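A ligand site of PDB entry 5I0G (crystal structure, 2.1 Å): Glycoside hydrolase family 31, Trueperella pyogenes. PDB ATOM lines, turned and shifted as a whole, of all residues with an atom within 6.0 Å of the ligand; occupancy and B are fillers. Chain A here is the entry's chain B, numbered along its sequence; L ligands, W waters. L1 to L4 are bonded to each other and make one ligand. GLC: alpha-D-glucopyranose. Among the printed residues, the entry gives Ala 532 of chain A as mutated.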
ATOM      1  N   HIS A  78      17.213  22.575 -18.705  1.00  0.00           N
ATOM      2  CA  HIS A  78      16.080  21.693 -18.425  1.00  0.00           C
ATOM      3  C   HIS A  78      14.872  22.549 -17.994  1.00  0.00           C
ATOM      4  O   HIS A  78      14.375  22.446 -16.863  1.00  0.00           O
ATOM      5  CB  HIS A  78      16.462  20.685 -17.327  1.00  0.00           C
ATOM      6  CG  HIS A  78      17.529  19.710 -17.762  1.00  0.00           C
ATOM      7  ND1 HIS A  78      17.291  18.710 -18.683  1.00  0.00           N
ATOM      8  CD2 HIS A  78      18.836  19.612 -17.433  1.00  0.00           C
ATOM      9  CE1 HIS A  78      18.397  18.031 -18.885  1.00  0.00           C
ATOM     10  NE2 HIS A  78      19.356  18.557 -18.129  1.00  0.00           N
ATOM     11  N   GLU A 198      28.312  19.590 -13.549  1.00  0.00           N
ATOM     12  CA  GLU A 198      27.635  19.469 -14.820  1.00  0.00           C
ATOM     13  C   GLU A 198      26.836  20.735 -15.104  1.00  0.00           C
ATOM     14  O   GLU A 198      25.735  20.914 -14.582  1.00  0.00           O
ATOM     15  CB  GLU A 198      26.707  18.252 -14.894  1.00  0.00           C
ATOM     16  CG  GLU A 198      26.221  18.070 -16.334  1.00  0.00           C
ATOM     17  CD  GLU A 198      24.944  17.282 -16.505  1.00  0.00           C
ATOM     18  OE1 GLU A 198      24.557  16.516 -15.585  1.00  0.00           O
ATOM     19  OE2 GLU A 198      24.339  17.412 -17.607  1.00  0.00           O
ATOM     20  N   TYR A 200      24.747  21.925 -17.826  1.00  0.00           N
ATOM     21  CA  TYR A 200      24.110  21.407 -19.015  1.00  0.00           C
ATOM     22  C   TYR A 200      23.849  22.559 -20.002  1.00  0.00           C
ATOM     23  O   TYR A 200      22.861  23.280 -19.909  1.00  0.00           O
ATOM     24  CB  TYR A 200      22.831  20.643 -18.678  1.00  0.00           C
ATOM     25  CG  TYR A 200      22.113  20.106 -19.891  1.00  0.00           C
ATOM     26  CD1 TYR A 200      22.698  19.147 -20.704  1.00  0.00           C
ATOM     27  CD2 TYR A 200      20.853  20.583 -20.239  1.00  0.00           C
ATOM     28  CE1 TYR A 200      22.046  18.659 -21.837  1.00  0.00           C
ATOM     29  CE2 TYR A 200      20.182  20.093 -21.347  1.00  0.00           C
ATOM     30  CZ  TYR A 200      20.772  19.136 -22.137  1.00  0.00           C
ATOM     31  OH  TYR A 200      20.113  18.675 -23.245  1.00  0.00           O
ATOM     32  N   TYR A 210      33.065  21.233 -16.753  1.00  0.00           N
ATOM     33  CA  TYR A 210      33.085  19.843 -16.347  1.00  0.00           C
ATOM     34  C   TYR A 210      34.507  19.404 -15.916  1.00  0.00           C
ATOM     35  O   TYR A 210      34.661  18.343 -15.278  1.00  0.00           O
ATOM     36  CB  TYR A 210      32.743  18.913 -17.500  1.00  0.00           C
ATOM     37  CG  TYR A 210      31.462  19.096 -18.259  1.00  0.00           C
ATOM     38  CD1 TYR A 210      31.427  19.875 -19.416  1.00  0.00           C
ATOM     39  CD2 TYR A 210      30.317  18.398 -17.890  1.00  0.00           C
ATOM     40  CE1 TYR A 210      30.256  20.013 -20.154  1.00  0.00           C
ATOM     41  CE2 TYR A 210      29.143  18.528 -18.631  1.00  0.00           C
ATOM     42  CZ  TYR A 210      29.122  19.328 -19.766  1.00  0.00           C
ATOM     43  OH  TYR A 210      27.972  19.436 -20.503  1.00  0.00           O
ATOM     44  N   ASN A 302      22.357   9.485 -30.563  1.00  0.00           N
ATOM     45  CA  ASN A 302      21.612   8.808 -29.520  1.00  0.00           C
ATOM     46  C   ASN A 302      20.427   7.982 -30.025  1.00  0.00           C
ATOM     47  O   ASN A 302      20.091   6.958 -29.436  1.00  0.00           O
ATOM     48  CB  ASN A 302      21.164   9.770 -28.434  1.00  0.00           C
ATOM     49  CG  ASN A 302      20.645   9.056 -27.215  1.00  0.00           C
ATOM     50  OD1 ASN A 302      19.433   8.882 -27.074  1.00  0.00           O
ATOM     51  ND2 ASN A 302      21.534   8.567 -26.345  1.00  0.00           N
ATOM     52  N   GLU A 330      25.239   4.806 -27.964  1.00  0.00           N
ATOM     53  CA  GLU A 330      24.752   5.236 -26.648  1.00  0.00           C
ATOM     54  C   GLU A 330      23.547   4.453 -26.167  1.00  0.00           C
ATOM     55  O   GLU A 330      23.537   3.942 -25.035  1.00  0.00           O
ATOM     56  CB  GLU A 330      24.426   6.713 -26.650  1.00  0.00           C
ATOM     57  CG  GLU A 330      25.640   7.590 -26.867  1.00  0.00           C
ATOM     58  CD  GLU A 330      25.380   9.017 -26.472  1.00  0.00           C
ATOM     59  OE1 GLU A 330      24.210   9.460 -26.520  1.00  0.00           O
ATOM     60  OE2 GLU A 330      26.358   9.700 -26.089  1.00  0.00           O
ATOM     61  N   ALA A 331      22.530   4.364 -27.037  1.00  0.00           N
ATOM     62  CA  ALA A 331      21.304   3.639 -26.704  1.00  0.00           C
ATOM     63  C   ALA A 331      21.395   2.168 -27.130  1.00  0.00           C
ATOM     64  O   ALA A 331      20.684   1.714 -28.049  1.00  0.00           O
ATOM     65  CB  ALA A 331      20.089   4.320 -27.330  1.00  0.00           C
ATOM     66  N   TRP A 332      22.260   1.442 -26.419  1.00  0.00           N
ATOM     67  CA  TRP A 332      22.563   0.030 -26.707  1.00  0.00           C
ATOM     68  C   TRP A 332      21.950  -0.973 -25.717  1.00  0.00           C
ATOM     69  O   TRP A 332      21.629  -2.120 -26.101  1.00  0.00           O
ATOM     70  CB  TRP A 332      24.081  -0.181 -26.770  1.00  0.00           C
ATOM     71  CG  TRP A 332      24.813  -0.005 -25.487  1.00  0.00           C
ATOM     72  CD1 TRP A 332      25.360   1.147 -25.016  1.00  0.00           C
ATOM     73  CD2 TRP A 332      25.129  -1.022 -24.526  1.00  0.00           C
ATOM     74  NE1 TRP A 332      25.977   0.925 -23.821  1.00  0.00           N
ATOM     75  CE2 TRP A 332      25.849  -0.390 -23.489  1.00  0.00           C
ATOM     76  CE3 TRP A 332      24.857  -2.384 -24.434  1.00  0.00           C
ATOM     77  CZ2 TRP A 332      26.332  -1.081 -22.381  1.00  0.00           C
ATOM     78  CZ3 TRP A 332      25.340  -3.091 -23.308  1.00  0.00           C
ATOM     79  CH2 TRP A 332      26.058  -2.428 -22.297  1.00  0.00           C
ATOM     80  N   GLU A 335      18.687   0.053 -20.672  1.00  0.00           N
ATOM     81  CA  GLU A 335      18.372   1.327 -20.004  1.00  0.00           C
ATOM     82  C   GLU A 335      18.046   1.185 -18.509  1.00  0.00           C
ATOM     83  O   GLU A 335      17.425   2.075 -17.910  1.00  0.00           O
ATOM     84  CB  GLU A 335      17.274   2.113 -20.759  1.00  0.00           C
ATOM     85  CG  GLU A 335      17.626   2.473 -22.207  1.00  0.00           C
ATOM     86  CD  GLU A 335      18.822   3.424 -22.327  1.00  0.00           C
ATOM     87  OE1 GLU A 335      18.952   4.365 -21.516  1.00  0.00           O
ATOM     88  OE2 GLU A 335      19.635   3.225 -23.249  1.00  0.00           O
ATOM     89  N   PHE A 338      22.819  -0.821 -17.861  1.00  0.00           N
ATOM     90  CA  PHE A 338      23.931  -0.443 -18.750  1.00  0.00           C
ATOM     91  C   PHE A 338      25.049  -1.487 -18.841  1.00  0.00           C
ATOM     92  O   PHE A 338      26.213  -1.157 -18.934  1.00  0.00           O
ATOM     93  CB  PHE A 338      24.443   0.970 -18.389  1.00  0.00           C
ATOM     94  CG  PHE A 338      23.348   1.984 -18.459  1.00  0.00           C
ATOM     95  CD1 PHE A 338      22.930   2.461 -19.686  1.00  0.00           C
ATOM     96  CD2 PHE A 338      22.654   2.367 -17.320  1.00  0.00           C
ATOM     97  CE1 PHE A 338      21.867   3.351 -19.782  1.00  0.00           C
ATOM     98  CE2 PHE A 338      21.600   3.260 -17.401  1.00  0.00           C
ATOM     99  CZ  PHE A 338      21.209   3.749 -18.626  1.00  0.00           C
ATOM    100  N   TRP A 387      28.475   3.475 -24.503  1.00  0.00           N
ATOM    101  CA  TRP A 387      28.218   4.473 -23.479  1.00  0.00           C
ATOM    102  C   TRP A 387      28.067   3.856 -22.096  1.00  0.00           C
ATOM    103  O   TRP A 387      27.603   2.715 -21.943  1.00  0.00           O
ATOM    104  CB  TRP A 387      26.962   5.218 -23.866  1.00  0.00           C
ATOM    105  CG  TRP A 387      26.608   6.439 -23.104  1.00  0.00           C
ATOM    106  CD1 TRP A 387      26.942   7.699 -23.412  1.00  0.00           C
ATOM    107  CD2 TRP A 387      25.753   6.515 -21.951  1.00  0.00           C
ATOM    108  NE1 TRP A 387      26.388   8.575 -22.517  1.00  0.00           N
ATOM    109  CE2 TRP A 387      25.655   7.862 -21.609  1.00  0.00           C
ATOM    110  CE3 TRP A 387      25.089   5.560 -21.178  1.00  0.00           C
ATOM    111  CZ2 TRP A 387      24.901   8.306 -20.524  1.00  0.00           C
ATOM    112  CZ3 TRP A 387      24.342   5.991 -20.094  1.00  0.00           C
ATOM    113  CH2 TRP A 387      24.263   7.371 -19.770  1.00  0.00           C
ATOM    114  N   LYS A 393      21.041   2.878 -11.074  1.00  0.00           N
ATOM    115  CA  LYS A 393      19.643   3.235 -10.813  1.00  0.00           C
ATOM    116  C   LYS A 393      18.987   2.320  -9.777  1.00  0.00           C
ATOM    117  O   LYS A 393      19.269   1.118  -9.755  1.00  0.00           O
ATOM    118  CB  LYS A 393      18.825   3.169 -12.104  1.00  0.00           C
ATOM    119  CG  LYS A 393      19.152   4.282 -13.071  1.00  0.00           C
ATOM    120  CD  LYS A 393      18.665   3.966 -14.475  1.00  0.00           C
ATOM    121  CE  LYS A 393      17.158   4.011 -14.586  1.00  0.00           C
ATOM    122  NZ  LYS A 393      16.792   3.805 -16.007  1.00  0.00           N
ATOM    123  N   TRP A 429      19.995  15.996 -10.490  1.00  0.00           N
ATOM    124  CA  TRP A 429      18.796  15.948 -11.334  1.00  0.00           C
ATOM    125  C   TRP A 429      18.888  14.798 -12.368  1.00  0.00           C
ATOM    126  O   TRP A 429      17.868  14.334 -12.861  1.00  0.00           O
ATOM    127  CB  TRP A 429      18.560  17.331 -12.021  1.00  0.00           C
ATOM    128  CG  TRP A 429      19.692  17.749 -12.916  1.00  0.00           C
ATOM    129  CD1 TRP A 429      19.869  17.388 -14.227  1.00  0.00           C
ATOM    130  CD2 TRP A 429      20.846  18.520 -12.544  1.00  0.00           C
ATOM    131  NE1 TRP A 429      21.047  17.911 -14.698  1.00  0.00           N
ATOM    132  CE2 TRP A 429      21.671  18.608 -13.695  1.00  0.00           C
ATOM    133  CE3 TRP A 429      21.263  19.148 -11.362  1.00  0.00           C
ATOM    134  CZ2 TRP A 429      22.897  19.296 -13.697  1.00  0.00           C
ATOM    135  CZ3 TRP A 429      22.478  19.854 -11.375  1.00  0.00           C
ATOM    136  CH2 TRP A 429      23.276  19.923 -12.540  1.00  0.00           C
ATOM    137  N   TRP A 430      20.100  14.336 -12.690  1.00  0.00           N
ATOM    138  CA  TRP A 430      20.297  13.229 -13.630  1.00  0.00           C
ATOM    139  C   TRP A 430      20.434  11.878 -12.908  1.00  0.00           C
ATOM    140  O   TRP A 430      21.366  11.692 -12.120  1.00  0.00           O
ATOM    141  CB  TRP A 430      21.545  13.496 -14.458  1.00  0.00           C
ATOM    142  CG  TRP A 430      21.643  12.708 -15.707  1.00  0.00           C
ATOM    143  CD1 TRP A 430      20.600  12.229 -16.453  1.00  0.00           C
ATOM    144  CD2 TRP A 430      22.839  12.331 -16.389  1.00  0.00           C
ATOM    145  NE1 TRP A 430      21.091  11.582 -17.563  1.00  0.00           N
ATOM    146  CE2 TRP A 430      22.453  11.631 -17.553  1.00  0.00           C
ATOM    147  CE3 TRP A 430      24.193  12.537 -16.151  1.00  0.00           C
ATOM    148  CZ2 TRP A 430      23.372  11.114 -18.459  1.00  0.00           C
ATOM    149  CZ3 TRP A 430      25.110  12.028 -17.045  1.00  0.00           C
ATOM    150  CH2 TRP A 430      24.697  11.323 -18.199  1.00  0.00           C
ATOM    151  N   PHE A 431      19.505  10.950 -13.205  1.00  0.00           N
ATOM    152  CA  PHE A 431      19.375   9.694 -12.467  1.00  0.00           C
ATOM    153  C   PHE A 431      19.307   9.996 -10.963  1.00  0.00           C
ATOM    154  O   PHE A 431      20.213   9.628 -10.202  1.00  0.00           O
ATOM    155  CB  PHE A 431      20.535   8.734 -12.775  1.00  0.00           C
ATOM    156  CG  PHE A 431      20.616   8.319 -14.223  1.00  0.00           C
ATOM    157  CD1 PHE A 431      19.628   7.515 -14.788  1.00  0.00           C
ATOM    158  CD2 PHE A 431      21.687   8.705 -14.995  1.00  0.00           C
ATOM    159  CE1 PHE A 431      19.709   7.103 -16.115  1.00  0.00           C
ATOM    160  CE2 PHE A 431      21.765   8.308 -16.330  1.00  0.00           C
ATOM    161  CZ  PHE A 431      20.794   7.503 -16.879  1.00  0.00           C
ATOM    162  N   LYS A 465      32.425   5.257 -23.799  1.00  0.00           N
ATOM    163  CA  LYS A 465      32.148   6.662 -23.612  1.00  0.00           C
ATOM    164  C   LYS A 465      31.711   6.745 -22.177  1.00  0.00           C
ATOM    165  O   LYS A 465      30.574   6.409 -21.835  1.00  0.00           O
ATOM    166  CB  LYS A 465      31.078   7.213 -24.582  1.00  0.00           C
ATOM    167  CG  LYS A 465      30.744   8.691 -24.357  1.00  0.00           C
ATOM    168  CD  LYS A 465      29.959   9.309 -25.509  1.00  0.00           C
ATOM    169  CE  LYS A 465      29.518  10.726 -25.164  1.00  0.00           C
ATOM    170  NZ  LYS A 465      28.546  11.321 -26.131  1.00  0.00           N
ATOM    171  N   ASP A 467      30.617   8.588 -19.640  1.00  0.00           N
ATOM    172  CA  ASP A 467      29.866   9.834 -19.495  1.00  0.00           C
ATOM    173  C   ASP A 467      29.630  10.123 -18.014  1.00  0.00           C
ATOM    174  O   ASP A 467      29.807   9.243 -17.186  1.00  0.00           O
ATOM    175  CB  ASP A 467      28.511   9.718 -20.216  1.00  0.00           C
ATOM    176  CG  ASP A 467      27.972  11.049 -20.715  1.00  0.00           C
ATOM    177  OD1 ASP A 467      28.276  12.116 -20.115  1.00  0.00           O
ATOM    178  OD2 ASP A 467      27.260  11.010 -21.741  1.00  0.00           O
ATOM    179  N   ARG A 516      33.667  13.450 -20.384  1.00  0.00           N
ATOM    180  CA  ARG A 516      33.446  14.895 -20.364  1.00  0.00           C
ATOM    181  C   ARG A 516      34.004  15.560 -19.109  1.00  0.00           C
ATOM    182  O   ARG A 516      34.406  16.731 -19.159  1.00  0.00           O
ATOM    183  CB  ARG A 516      31.972  15.236 -20.530  1.00  0.00           C
ATOM    184  CG  ARG A 516      31.092  14.796 -19.367  1.00  0.00           C
ATOM    185  CD  ARG A 516      29.633  15.039 -19.614  1.00  0.00           C
ATOM    186  NE  ARG A 516      28.888  14.968 -18.364  1.00  0.00           N
ATOM    187  CZ  ARG A 516      27.568  14.855 -18.263  1.00  0.00           C
ATOM    188  NH1 ARG A 516      26.792  14.720 -19.334  1.00  0.00           N
ATOM    189  NH2 ARG A 516      27.006  14.852 -17.069  1.00  0.00           N
ATOM    190  N   TRP A 529      35.759  15.091 -24.460  1.00  0.00           N
ATOM    191  CA  TRP A 529      34.965  15.988 -25.315  1.00  0.00           C
ATOM    192  C   TRP A 529      34.338  17.105 -24.472  1.00  0.00           C
ATOM    193  O   TRP A 529      34.187  16.969 -23.259  1.00  0.00           O
ATOM    194  CB  TRP A 529      33.935  15.217 -26.195  1.00  0.00           C
ATOM    195  CG  TRP A 529      32.524  15.099 -25.671  1.00  0.00           C
ATOM    196  CD1 TRP A 529      31.426  15.786 -26.109  1.00  0.00           C
ATOM    197  CD2 TRP A 529      32.060  14.194 -24.658  1.00  0.00           C
ATOM    198  NE1 TRP A 529      30.308  15.405 -25.397  1.00  0.00           N
ATOM    199  CE2 TRP A 529      30.662  14.424 -24.512  1.00  0.00           C
ATOM    200  CE3 TRP A 529      32.669  13.209 -23.882  1.00  0.00           C
ATOM    201  CZ2 TRP A 529      29.880  13.713 -23.590  1.00  0.00           C
ATOM    202  CZ3 TRP A 529      31.876  12.492 -22.966  1.00  0.00           C
ATOM    203  CH2 TRP A 529      30.509  12.768 -22.820  1.00  0.00           C
ATOM    204  N   GLY A 531      31.426  18.367 -23.975  1.00  0.00           N
ATOM    205  CA  GLY A 531      30.131  18.243 -23.319  1.00  0.00           C
ATOM    206  C   GLY A 531      28.981  18.714 -24.174  1.00  0.00           C
ATOM    207  O   GLY A 531      29.064  18.718 -25.387  1.00  0.00           O
ATOM    208  N   ALA A 532      27.908  19.117 -23.526  1.00  0.00           N
ATOM    209  CA  ALA A 532      26.642  19.365 -24.200  1.00  0.00           C
ATOM    210  C   ALA A 532      26.514  20.837 -24.576  1.00  0.00           C
ATOM    211  O   ALA A 532      26.737  21.703 -23.733  1.00  0.00           O
ATOM    212  CB  ALA A 532      25.495  18.947 -23.290  1.00  0.00           C
ATOM    213  N   ASP A 561      31.258  17.877 -29.929  1.00  0.00           N
ATOM    214  CA  ASP A 561      30.121  17.546 -30.789  1.00  0.00           C
ATOM    215  C   ASP A 561      30.052  18.625 -31.849  1.00  0.00           C
ATOM    216  O   ASP A 561      29.519  19.724 -31.587  1.00  0.00           O
ATOM    217  CB  ASP A 561      28.803  17.530 -30.009  1.00  0.00           C
ATOM    218  CG  ASP A 561      28.797  16.539 -28.871  1.00  0.00           C
ATOM    219  OD1 ASP A 561      29.590  15.563 -28.908  1.00  0.00           O
ATOM    220  OD2 ASP A 561      27.994  16.756 -27.919  1.00  0.00           O
ATOM    221  N   PHE A 565      25.039  19.291 -30.574  1.00  0.00           N
ATOM    222  CA  PHE A 565      24.241  18.058 -30.536  1.00  0.00           C
ATOM    223  C   PHE A 565      22.772  18.269 -30.137  1.00  0.00           C
ATOM    224  O   PHE A 565      21.954  17.389 -30.392  1.00  0.00           O
ATOM    225  CB  PHE A 565      24.955  16.976 -29.643  1.00  0.00           C
ATOM    226  CG  PHE A 565      24.394  16.810 -28.233  1.00  0.00           C
ATOM    227  CD1 PHE A 565      24.278  17.884 -27.345  1.00  0.00           C
ATOM    228  CD2 PHE A 565      24.036  15.541 -27.782  1.00  0.00           C
ATOM    229  CE1 PHE A 565      23.768  17.700 -26.062  1.00  0.00           C
ATOM    230  CE2 PHE A 565      23.542  15.340 -26.497  1.00  0.00           C
ATOM    231  CZ  PHE A 565      23.400  16.419 -25.629  1.00  0.00           C
ATOM    232  N   HIS A 591      27.539  14.224 -33.312  1.00  0.00           N
ATOM    233  CA  HIS A 591      26.697  13.628 -32.279  1.00  0.00           C
ATOM    234  C   HIS A 591      25.325  14.303 -32.256  1.00  0.00           C
ATOM    235  O   HIS A 591      25.194  15.436 -32.706  1.00  0.00           O
ATOM    236  CB  HIS A 591      27.419  13.773 -30.931  1.00  0.00           C
ATOM    237  CG  HIS A 591      26.697  13.141 -29.782  1.00  0.00           C
ATOM    238  ND1 HIS A 591      26.092  11.908 -29.867  1.00  0.00           N
ATOM    239  CD2 HIS A 591      26.507  13.576 -28.515  1.00  0.00           C
ATOM    240  CE1 HIS A 591      25.521  11.623 -28.716  1.00  0.00           C
ATOM    241  NE2 HIS A 591      25.771  12.602 -27.872  1.00  0.00           N
ATOM    242  N   SER A 592      24.308  13.604 -31.750  1.00  0.00           N
ATOM    243  CA  SER A 592      22.964  14.156 -31.655  1.00  0.00           C
ATOM    244  C   SER A 592      22.224  13.620 -30.417  1.00  0.00           C
ATOM    245  O   SER A 592      22.345  12.441 -30.079  1.00  0.00           O
ATOM    246  CB  SER A 592      22.143  13.815 -32.920  1.00  0.00           C
ATOM    247  OG  SER A 592      21.998  12.404 -33.063  1.00  0.00           O
ATOM    248  N   GLU A 593      21.453  14.496 -29.791  1.00  0.00           N
ATOM    249  CA  GLU A 593      20.762  14.207 -28.545  1.00  0.00           C
ATOM    250  C   GLU A 593      19.472  13.415 -28.755  1.00  0.00           C
ATOM    251  O   GLU A 593      18.857  13.500 -29.815  1.00  0.00           O
ATOM    252  CB  GLU A 593      20.396  15.527 -27.864  1.00  0.00           C
ATOM    253  CG  GLU A 593      20.034  15.363 -26.399  1.00  0.00           C
ATOM    254  CD  GLU A 593      19.743  16.678 -25.712  1.00  0.00           C
ATOM    255  OE1 GLU A 593      19.258  17.614 -26.406  1.00  0.00           O
ATOM    256  OE2 GLU A 593      19.992  16.723 -24.480  1.00  0.00           O
ATOM    257  N   PHE A 594      19.065  12.674 -27.727  1.00  0.00           N
ATOM    258  CA  PHE A 594      17.733  12.014 -27.672  1.00  0.00           C
ATOM    259  C   PHE A 594      16.600  13.019 -27.935  1.00  0.00           C
ATOM    260  O   PHE A 594      16.605  14.109 -27.401  1.00  0.00           O
ATOM    261  CB  PHE A 594      17.482  11.338 -26.309  1.00  0.00           C
ATOM    262  CG  PHE A 594      16.248  10.474 -26.272  1.00  0.00           C
ATOM    263  CD1 PHE A 594      16.176   9.300 -27.013  1.00  0.00           C
ATOM    264  CD2 PHE A 594      15.139  10.840 -25.482  1.00  0.00           C
ATOM    265  CE1 PHE A 594      15.028   8.499 -26.984  1.00  0.00           C
ATOM    266  CE2 PHE A 594      13.991  10.039 -25.453  1.00  0.00           C
ATOM    267  CZ  PHE A 594      13.935   8.872 -26.198  1.00  0.00           C
HETATM  268  C1  GLC L   1      19.841  14.702 -20.582  1.00  0.00           C
HETATM  269  C2  GLC L   1      21.028  14.683 -21.550  1.00  0.00           C
HETATM  270  C3  GLC L   1      22.319  14.227 -20.846  1.00  0.00           C
HETATM  271  C4  GLC L   1      22.554  15.136 -19.629  1.00  0.00           C
HETATM  272  C5  GLC L   1      21.329  15.048 -18.731  1.00  0.00           C
HETATM  273  C6  GLC L   1      21.461  15.757 -17.379  1.00  0.00           C
HETATM  274  O2  GLC L   1      20.737  13.821 -22.658  1.00  0.00           O
HETATM  275  O3  GLC L   1      23.381  14.307 -21.819  1.00  0.00           O
HETATM  276  O4  GLC L   1      23.724  14.757 -18.900  1.00  0.00           O
HETATM  277  O5  GLC L   1      20.183  15.531 -19.461  1.00  0.00           O
HETATM  278  O6  GLC L   1      21.777  17.141 -17.514  1.00  0.00           O
HETATM  279  C1  GLC L   2      24.425  13.328 -21.673  1.00  0.00           C
HETATM  280  C2  GLC L   2      25.592  13.648 -22.609  1.00  0.00           C
HETATM  281  C3  GLC L   2      25.208  13.357 -24.055  1.00  0.00           C
HETATM  282  C4  GLC L   2      24.608  11.967 -24.238  1.00  0.00           C
HETATM  283  C5  GLC L   2      23.502  11.734 -23.227  1.00  0.00           C
HETATM  284  C6  GLC L   2      23.004  10.306 -23.270  1.00  0.00           C
HETATM  285  O2  GLC L   2      25.984  15.025 -22.509  1.00  0.00           O
HETATM  286  O3  GLC L   2      26.338  13.479 -24.927  1.00  0.00           O
HETATM  287  O4  GLC L   2      24.066  11.871 -25.550  1.00  0.00           O
HETATM  288  O5  GLC L   2      23.964  12.002 -21.887  1.00  0.00           O
HETATM  289  O6  GLC L   2      21.743  10.304 -22.586  1.00  0.00           O
HETATM  290  C1  GLC L   3      18.338   9.491 -19.274  1.00  0.00           C
HETATM  291  C2  GLC L   3      17.030   9.209 -18.537  1.00  0.00           C
HETATM  292  C3  GLC L   3      15.965  10.213 -18.959  1.00  0.00           C
HETATM  293  C4  GLC L   3      16.466  11.635 -18.742  1.00  0.00           C
HETATM  294  C5  GLC L   3      17.728  11.837 -19.557  1.00  0.00           C
HETATM  295  C6  GLC L   3      18.315  13.247 -19.419  1.00  0.00           C
HETATM  296  O2  GLC L   3      16.599   7.861 -18.810  1.00  0.00           O
HETATM  297  O3  GLC L   3      14.783  10.018 -18.177  1.00  0.00           O
HETATM  298  O4  GLC L   3      15.449  12.559 -19.141  1.00  0.00           O
HETATM  299  O5  GLC L   3      18.709  10.873 -19.137  1.00  0.00           O
HETATM  300  O6  GLC L   3      19.508  13.348 -20.228  1.00  0.00           O
HETATM  301  C1  GLC L   4      20.704   9.664 -23.354  1.00  0.00           C
HETATM  302  C2  GLC L   4      19.411   9.807 -22.574  1.00  0.00           C
HETATM  303  C3  GLC L   4      19.473   8.988 -21.296  1.00  0.00           C
HETATM  304  C4  GLC L   4      19.797   7.532 -21.607  1.00  0.00           C
HETATM  305  C5  GLC L   4      21.074   7.456 -22.466  1.00  0.00           C
HETATM  306  C6  GLC L   4      21.376   6.053 -22.971  1.00  0.00           C
HETATM  307  O2  GLC L   4      19.242  11.185 -22.253  1.00  0.00           O
HETATM  308  O3  GLC L   4      18.201   9.091 -20.648  1.00  0.00           O
HETATM  309  O4  GLC L   4      19.953   6.828 -20.366  1.00  0.00           O
HETATM  310  O5  GLC L   4      20.949   8.288 -23.624  1.00  0.00           O
HETATM  311  O6  GLC L   4      20.450   5.701 -24.006  1.00  0.00           O
HETATM  312  O   HOH W   1      18.446   7.038 -25.088  1.00  0.00           O
HETATM  313  O   HOH W   2      20.957  12.295 -25.714  1.00  0.00           O
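OE2 of Glu 198 lies within hydrogen-bond range of O6 of GLC L1, at 2.6 Å.
The side-chain carboxylate of Glu 330 is in hydrogen-bond range of an oxygen (O4) of GLC L2, at 2.6 Å.
The side-chain carboxylate (OE2) of Glu 335 sits at hydrogen-bond distance from an oxygen (O6) of GLC L4, 2.7 Å away.
O5 of GLC L4 lies within hydrogen-bond range of ND2 of Asn 302 (2.8 Å).
O6 of GLC L1 lies within hydrogen-bond range of NE2 of His 78 (2.9 Å).
An oxygen (O5) of GLC L3 lies within hydrogen-bond range of the indole nitrogen (NE1) of Trp 430, at 2.9 Å.
A ring nitrogen (NE2) of His 591 is in hydrogen-bond range of an oxygen (O4) of GLC L2, 3.0 Å away.
NE1 of Trp 429 lies within hydrogen-bond range of O6 of GLC L1, at 3.0 Å.
The guanidinium group (NH1) of Arg 516 lies within hydrogen-bond range of an oxygen (O4) of GLC L1.
The side-chain amino group of Lys 465 is in hydrogen-bond range of an oxygen (O3) of GLC L2 (3.3 Å).
The side-chain carboxylate of Glu 198 is in salt-bridge range of the guanidinium group of Arg 516 (3.3 Å).
The side-chain amide nitrogen (ND2) of Asn 302 is in hydrogen-bond range of the side-chain carboxylate (OE1) of Glu 330 (2.8 Å).
The side-chain amino group of Lys 465 lies within salt-bridge range of the side-chain carboxylate of Glu 330.
O of Glu 335 is in hydrogen-bond range of NZ of Lys 393, at 2.6 Å.
OD2 of Asp 467 is in hydrogen-bond range of NE1 of Trp 387 (2.7 Å).
N of Glu 593 lies within hydrogen-bond range of O of Phe 565 (3.0 Å).
The side-chain carboxylate (OE1) of Glu 593 sits close to the side-chain hydroxyl (OH) of Tyr 200 (3.4 Å).
The backbone carbonyl oxygen of Trp 387 is in hydrogen-bond range of the indole nitrogen of Trp 332 (3.1 Å).
O5 of GLC L2 sits close to OD2 of Asp 467.
CG of Tyr 200 touches O6 of GLC L1, at 3.8 Å.
Ala 331 touches the ligand.
CZ of Phe 338 touches O4 of GLC L4, at 3.8 Å.
Trp 387 touches the ligand.
CZ of Phe 431 touches O4 of GLC L4, at 3.6 Å.
CZ2 of Trp 529 touches O3 of GLC L2, at 3.8 Å.
CE2 of Phe 565 touches C3 of GLC L2 (3.6 Å).
OE2 of Glu 593 touches O2 of GLC L1, at 3.5 Å.
Hydrophobic or aromatic side chains that line the ligand: His 78, Tyr 200, Ala 331, Phe 338, Trp 387, Trp 429, Trp 430, Phe 431, Trp 529, Phe 565 and His 591.
Of the 27 residues printed, 19 come within 4 Å of the ligand.
The nearest printed residue that does not touch the ligand is Ala 532 (4.03 Å).
Water W1 bridges an oxygen (O6) of GLC L4 (2.6 Å) and the side-chain amide oxygen (OD1) of Asn 302 (2.9 Å).
Water W2 bridges N of Phe 594 and O4 of GLC L2.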
